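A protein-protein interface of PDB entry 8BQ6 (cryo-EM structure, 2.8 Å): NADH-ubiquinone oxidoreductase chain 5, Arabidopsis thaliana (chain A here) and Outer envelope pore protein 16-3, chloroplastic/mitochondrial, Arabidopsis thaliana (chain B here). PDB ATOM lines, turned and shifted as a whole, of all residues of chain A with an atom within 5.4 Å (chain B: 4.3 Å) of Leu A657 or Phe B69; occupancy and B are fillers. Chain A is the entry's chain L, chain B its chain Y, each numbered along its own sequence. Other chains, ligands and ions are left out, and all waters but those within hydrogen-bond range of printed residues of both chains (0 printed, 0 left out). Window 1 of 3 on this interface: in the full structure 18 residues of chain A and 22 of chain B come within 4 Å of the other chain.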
ATOM      1  N   ARG A 652      30.425  15.626  13.613  1.00  0.00           N
ATOM      2  CA  ARG A 652      29.496  16.562  14.243  1.00  0.00           C
ATOM      3  C   ARG A 652      28.149  16.571  13.529  1.00  0.00           C
ATOM      4  O   ARG A 652      27.096  16.421  14.157  1.00  0.00           O
ATOM      5  CB  ARG A 652      30.093  17.970  14.253  1.00  0.00           C
ATOM      6  CG  ARG A 652      31.588  18.027  14.488  1.00  0.00           C
ATOM      7  CD  ARG A 652      31.907  18.769  15.772  1.00  0.00           C
ATOM      8  NE  ARG A 652      31.125  19.994  15.897  1.00  0.00           N
ATOM      9  CZ  ARG A 652      31.474  21.160  15.371  1.00  0.00           C
ATOM     10  NH1 ARG A 652      32.572  21.291  14.646  1.00  0.00           N
ATOM     11  NH2 ARG A 652      30.694  22.219  15.571  1.00  0.00           N
ATOM     12  N   LEU A 653      28.171  16.739  12.204  1.00  0.00           N
ATOM     13  CA  LEU A 653      26.934  16.829  11.433  1.00  0.00           C
ATOM     14  C   LEU A 653      26.055  15.604  11.661  1.00  0.00           C
ATOM     15  O   LEU A 653      24.841  15.727  11.864  1.00  0.00           O
ATOM     16  CB  LEU A 653      27.242  16.986   9.941  1.00  0.00           C
ATOM     17  CG  LEU A 653      27.951  18.278   9.530  1.00  0.00           C
ATOM     18  CD1 LEU A 653      28.325  18.237   8.055  1.00  0.00           C
ATOM     19  CD2 LEU A 653      27.084  19.490   9.834  1.00  0.00           C
ATOM     20  N   SER A 654      26.663  14.415  11.667  1.00  0.00           N
ATOM     21  CA  SER A 654      25.926  13.160  11.738  1.00  0.00           C
ATOM     22  C   SER A 654      25.026  13.086  12.968  1.00  0.00           C
ATOM     23  O   SER A 654      23.818  12.847  12.856  1.00  0.00           O
ATOM     24  CB  SER A 654      26.918  11.990  11.726  1.00  0.00           C
ATOM     25  OG  SER A 654      26.409  10.872  12.431  1.00  0.00           O
ATOM     26  N   PHE A 655      25.602  13.319  14.149  1.00  0.00           N
ATOM     27  CA  PHE A 655      24.811  13.286  15.376  1.00  0.00           C
ATOM     28  C   PHE A 655      23.828  14.446  15.432  1.00  0.00           C
ATOM     29  O   PHE A 655      22.739  14.315  16.003  1.00  0.00           O
ATOM     30  CB  PHE A 655      25.727  13.303  16.597  1.00  0.00           C
ATOM     31  CG  PHE A 655      26.844  12.312  16.522  1.00  0.00           C
ATOM     32  CD1 PHE A 655      26.589  10.957  16.622  1.00  0.00           C
ATOM     33  CD2 PHE A 655      28.148  12.734  16.351  1.00  0.00           C
ATOM     34  CE1 PHE A 655      27.614  10.040  16.550  1.00  0.00           C
ATOM     35  CE2 PHE A 655      29.179  11.823  16.271  1.00  0.00           C
ATOM     36  CZ  PHE A 655      28.912  10.473  16.373  1.00  0.00           C
ATOM     37  N   ILE A 656      24.199  15.594  14.860  1.00  0.00           N
ATOM     38  CA  ILE A 656      23.268  16.716  14.802  1.00  0.00           C
ATOM     39  C   ILE A 656      21.990  16.301  14.083  1.00  0.00           C
ATOM     40  O   ILE A 656      20.879  16.548  14.564  1.00  0.00           O
ATOM     41  CB  ILE A 656      23.926  17.935  14.128  1.00  0.00           C
ATOM     42  CG1 ILE A 656      25.042  18.515  15.006  1.00  0.00           C
ATOM     43  CG2 ILE A 656      22.889  18.993  13.803  1.00  0.00           C
ATOM     44  CD1 ILE A 656      24.712  18.581  16.490  1.00  0.00           C
ATOM     45  N   LEU A 657      22.130  15.629  12.938  1.00  0.00           N
ATOM     46  CA  LEU A 657      20.965  15.293  12.129  1.00  0.00           C
ATOM     47  C   LEU A 657      20.085  14.250  12.812  1.00  0.00           C
ATOM     48  O   LEU A 657      18.855  14.289  12.683  1.00  0.00           O
ATOM     49  CB  LEU A 657      21.410  14.807  10.751  1.00  0.00           C
ATOM     50  CG  LEU A 657      22.058  15.868   9.854  1.00  0.00           C
ATOM     51  CD1 LEU A 657      23.318  15.330   9.205  1.00  0.00           C
ATOM     52  CD2 LEU A 657      21.094  16.365   8.796  1.00  0.00           C
ATOM     53  N   ILE A 658      20.693  13.313  13.544  1.00  0.00           N
ATOM     54  CA  ILE A 658      19.917  12.277  14.223  1.00  0.00           C
ATOM     55  C   ILE A 658      19.022  12.897  15.287  1.00  0.00           C
ATOM     56  O   ILE A 658      17.838  12.561  15.401  1.00  0.00           O
ATOM     57  CB  ILE A 658      20.851  11.209  14.820  1.00  0.00           C
ATOM     58  CG1 ILE A 658      21.493  10.382  13.706  1.00  0.00           C
ATOM     59  CG2 ILE A 658      20.088  10.300  15.766  1.00  0.00           C
ATOM     60  CD1 ILE A 658      20.519   9.947  12.640  1.00  0.00           C
ATOM     61  N   VAL A 659      19.573  13.819  16.077  1.00  0.00           N
ATOM     62  CA  VAL A 659      18.770  14.503  17.086  1.00  0.00           C
ATOM     63  C   VAL A 659      17.748  15.418  16.422  1.00  0.00           C
ATOM     64  O   VAL A 659      16.599  15.519  16.869  1.00  0.00           O
ATOM     65  CB  VAL A 659      19.685  15.271  18.061  1.00  0.00           C
ATOM     66  CG1 VAL A 659      19.012  16.543  18.552  1.00  0.00           C
ATOM     67  CG2 VAL A 659      20.068  14.384  19.231  1.00  0.00           C
ATOM     68  N   SER A 660      18.142  16.083  15.332  1.00  0.00           N
ATOM     69  CA  SER A 660      17.223  16.982  14.639  1.00  0.00           C
ATOM     70  C   SER A 660      16.055  16.234  14.019  1.00  0.00           C
ATOM     71  O   SER A 660      15.004  16.829  13.758  1.00  0.00           O
ATOM     72  CB  SER A 660      17.957  17.762  13.555  1.00  0.00           C
ATOM     73  OG  SER A 660      17.017  18.391  12.704  1.00  0.00           O
ATOM     74  N   SER A 661      16.222  14.939  13.759  1.00  0.00           N
ATOM     75  CA  SER A 661      15.131  14.157  13.192  1.00  0.00           C
ATOM     76  C   SER A 661      13.946  14.084  14.145  1.00  0.00           C
ATOM     77  O   SER A 661      12.817  13.819  13.716  1.00  0.00           O
ATOM     78  CB  SER A 661      15.635  12.759  12.851  1.00  0.00           C
ATOM     79  OG  SER A 661      16.906  12.841  12.230  1.00  0.00           O
ATOM     80  N   THR A 664      10.295  16.519  13.737  1.00  0.00           N
ATOM     81  CA  THR A 664       9.735  16.352  12.404  1.00  0.00           C
ATOM     82  C   THR A 664       8.239  16.099  12.520  1.00  0.00           C
ATOM     83  O   THR A 664       7.811  15.230  13.287  1.00  0.00           O
ATOM     84  CB  THR A 664      10.419  15.201  11.653  1.00  0.00           C
ATOM     85  OG1 THR A 664      11.697  15.638  11.173  1.00  0.00           O
ATOM     86  CG2 THR A 664       9.572  14.743  10.477  1.00  0.00           C
ATOM     87  N   GLY B  26      23.822  16.664   4.178  1.00  0.00           N
ATOM     88  CA  GLY B  26      22.502  16.807   4.760  1.00  0.00           C
ATOM     89  C   GLY B  26      21.406  16.372   3.812  1.00  0.00           C
ATOM     90  O   GLY B  26      20.471  15.678   4.212  1.00  0.00           O
ATOM     91  N   ALA B  29      21.428  12.459   3.631  1.00  0.00           N
ATOM     92  CA  ALA B  29      20.849  11.856   4.827  1.00  0.00           C
ATOM     93  C   ALA B  29      19.347  12.108   4.905  1.00  0.00           C
ATOM     94  O   ALA B  29      18.585  11.229   5.326  1.00  0.00           O
ATOM     95  CB  ALA B  29      21.553  12.388   6.074  1.00  0.00           C
ATOM     96  N   GLY B  30      18.901  13.303   4.514  1.00  0.00           N
ATOM     97  CA  GLY B  30      17.478  13.594   4.515  1.00  0.00           C
ATOM     98  C   GLY B  30      16.712  12.792   3.484  1.00  0.00           C
ATOM     99  O   GLY B  30      15.562  12.413   3.713  1.00  0.00           O
ATOM    100  N   TYR B  33      16.413   9.330   5.061  1.00  0.00           N
ATOM    101  CA  TYR B  33      15.436   9.381   6.145  1.00  0.00           C
ATOM    102  C   TYR B  33      14.015   9.482   5.601  1.00  0.00           C
ATOM    103  O   TYR B  33      13.096   8.827   6.111  1.00  0.00           O
ATOM    104  CB  TYR B  33      15.757  10.578   7.034  1.00  0.00           C
ATOM    105  CG  TYR B  33      14.824  10.829   8.191  1.00  0.00           C
ATOM    106  CD1 TYR B  33      14.429  12.116   8.498  1.00  0.00           C
ATOM    107  CD2 TYR B  33      14.414   9.804   9.029  1.00  0.00           C
ATOM    108  CE1 TYR B  33      13.607  12.379   9.566  1.00  0.00           C
ATOM    109  CE2 TYR B  33      13.595  10.061  10.112  1.00  0.00           C
ATOM    110  CZ  TYR B  33      13.189  11.352  10.370  1.00  0.00           C
ATOM    111  OH  TYR B  33      12.369  11.636  11.438  1.00  0.00           O
ATOM    112  N   HIS B  65      12.345  16.040   2.976  1.00  0.00           N
ATOM    113  CA  HIS B  65      13.288  15.734   4.044  1.00  0.00           C
ATOM    114  C   HIS B  65      14.720  16.026   3.618  1.00  0.00           C
ATOM    115  O   HIS B  65      15.521  16.512   4.426  1.00  0.00           O
ATOM    116  CB  HIS B  65      13.118  14.289   4.501  1.00  0.00           C
ATOM    117  CG  HIS B  65      12.084  14.136   5.570  1.00  0.00           C
ATOM    118  ND1 HIS B  65      10.761  13.873   5.293  1.00  0.00           N
ATOM    119  CD2 HIS B  65      12.169  14.262   6.914  1.00  0.00           C
ATOM    120  CE1 HIS B  65      10.081  13.820   6.423  1.00  0.00           C
ATOM    121  NE2 HIS B  65      10.912  14.052   7.422  1.00  0.00           N
ATOM    122  N   GLY B  66      15.058  15.770   2.352  1.00  0.00           N
ATOM    123  CA  GLY B  66      16.366  16.162   1.863  1.00  0.00           C
ATOM    124  C   GLY B  66      16.594  17.656   1.976  1.00  0.00           C
ATOM    125  O   GLY B  66      17.673  18.097   2.371  1.00  0.00           O
ATOM    126  N   LEU B  67      15.566  18.450   1.670  1.00  0.00           N
ATOM    127  CA  LEU B  67      15.686  19.902   1.756  1.00  0.00           C
ATOM    128  C   LEU B  67      15.897  20.358   3.193  1.00  0.00           C
ATOM    129  O   LEU B  67      16.796  21.160   3.475  1.00  0.00           O
ATOM    130  CB  LEU B  67      14.441  20.568   1.176  1.00  0.00           C
ATOM    131  CG  LEU B  67      14.566  21.081  -0.256  1.00  0.00           C
ATOM    132  CD1 LEU B  67      15.469  22.304  -0.317  1.00  0.00           C
ATOM    133  CD2 LEU B  67      15.094  19.974  -1.141  1.00  0.00           C
ATOM    134  N   THR B  68      15.053  19.887   4.115  1.00  0.00           N
ATOM    135  CA  THR B  68      15.196  20.356   5.490  1.00  0.00           C
ATOM    136  C   THR B  68      16.525  19.911   6.087  1.00  0.00           C
ATOM    137  O   THR B  68      17.210  20.700   6.752  1.00  0.00           O
ATOM    138  CB  THR B  68      14.027  19.892   6.361  1.00  0.00           C
ATOM    139  OG1 THR B  68      14.336  20.141   7.738  1.00  0.00           O
ATOM    140  CG2 THR B  68      13.760  18.425   6.181  1.00  0.00           C
ATOM    141  N   PHE B  69      16.929  18.663   5.832  1.00  0.00           N
ATOM    142  CA  PHE B  69      18.204  18.203   6.363  1.00  0.00           C
ATOM    143  C   PHE B  69      19.373  18.940   5.722  1.00  0.00           C
ATOM    144  O   PHE B  69      20.372  19.201   6.395  1.00  0.00           O
ATOM    145  CB  PHE B  69      18.340  16.692   6.179  1.00  0.00           C
ATOM    146  CG  PHE B  69      17.704  15.879   7.280  1.00  0.00           C
ATOM    147  CD1 PHE B  69      16.504  16.270   7.848  1.00  0.00           C
ATOM    148  CD2 PHE B  69      18.302  14.713   7.733  1.00  0.00           C
ATOM    149  CE1 PHE B  69      15.921  15.521   8.853  1.00  0.00           C
ATOM    150  CE2 PHE B  69      17.722  13.961   8.738  1.00  0.00           C
ATOM    151  CZ  PHE B  69      16.534  14.370   9.301  1.00  0.00           C
ATOM    152  N   ALA B  70      19.270  19.296   4.437  1.00  0.00           N
ATOM    153  CA  ALA B  70      20.332  20.065   3.802  1.00  0.00           C
ATOM    154  C   ALA B  70      20.437  21.454   4.408  1.00  0.00           C
ATOM    155  O   ALA B  70      21.541  21.958   4.636  1.00  0.00           O
ATOM    156  CB  ALA B  70      20.094  20.157   2.296  1.00  0.00           C
ATOM    157  N   ALA B  71      19.295  22.089   4.678  1.00  0.00           N
ATOM    158  CA  ALA B  71      19.314  23.394   5.327  1.00  0.00           C
ATOM    159  C   ALA B  71      19.990  23.318   6.690  1.00  0.00           C
ATOM    160  O   ALA B  71      20.839  24.155   7.019  1.00  0.00           O
ATOM    161  CB  ALA B  71      17.893  23.938   5.454  1.00  0.00           C
ATOM    162  N   ILE B  72      19.638  22.313   7.498  1.00  0.00           N
ATOM    163  CA  ILE B  72      20.298  22.183   8.798  1.00  0.00           C
ATOM    164  C   ILE B  72      21.796  21.955   8.616  1.00  0.00           C
ATOM    165  O   ILE B  72      22.627  22.676   9.184  1.00  0.00           O
ATOM    166  CB  ILE B  72      19.665  21.056   9.634  1.00  0.00           C
ATOM    167  CG1 ILE B  72      18.143  21.107   9.579  1.00  0.00           C
ATOM    168  CG2 ILE B  72      20.136  21.145  11.071  1.00  0.00           C
ATOM    169  CD1 ILE B  72      17.489  19.784   9.931  1.00  0.00           C
ATOM    170  N   GLY B  73      22.161  20.966   7.796  1.00  0.00           N
ATOM    171  CA  GLY B  73      23.556  20.597   7.634  1.00  0.00           C
ATOM    172  C   GLY B  73      24.400  21.647   6.949  1.00  0.00           C
ATOM    173  O   GLY B  73      25.629  21.569   7.004  1.00  0.00           O
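O of Ser A661 sits at hydrogen-bond distance from OH of Tyr B33, 3.2 Å away.
Printed residues of chain B that touch a printed residue of chain A: Tyr B33, His B65, Phe B69, Ile B72 and Gly B73.
Printed residues of chain A that touch a printed residue of chain B: Leu A653, Leu A657, Ser A660, Ser A661 and Thr A664.
Hydrophobic or aromatic side chains of chain A within 4 Å of the printed part of chain B: Leu A653 and Leu A657.
Among the printed residues, no Asp or Glu carboxylate lies within 4 Å of a Lys or Arg side-chain nitrogen of the other chain.
The side-chain hydroxyl (OG1) of Thr A664 is in hydrogen-bond range of the backbone carbonyl oxygen (O) of Ser A661 (3.3 Å).
O of Leu A657 lies within hydrogen-bond range of OG of Ser A661, at 2.5 Å.
O of Ile A658 is in hydrogen-bond range of OG of Ser A661 (3.3 Å).
Leu A657 touches just one residue of chain B: Phe B69.
Phe B69 touches just these residues of chain A: Leu A657 and Ser A661.
Of the printed residues of chain B, Thr A664 touches His B65 (3.4 Å).
Printed residues of chain B within 4 Å of Ser A661: Tyr B33 and Phe B69.
Of the printed residues of chain B, Ser A660 touches Ile B72 (3.1 Å).
The nearest printed residue of chain B that does not touch Ser A661 is Ile B72 (6.3 Å).
Among the printed residues, pairs that only touch across the chains: Leu A653 with Gly B73, Leu A657 with Phe B69, Ser A660 with Ile B72, Ser A661 with Phe B69 and Thr A664 with His B65.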
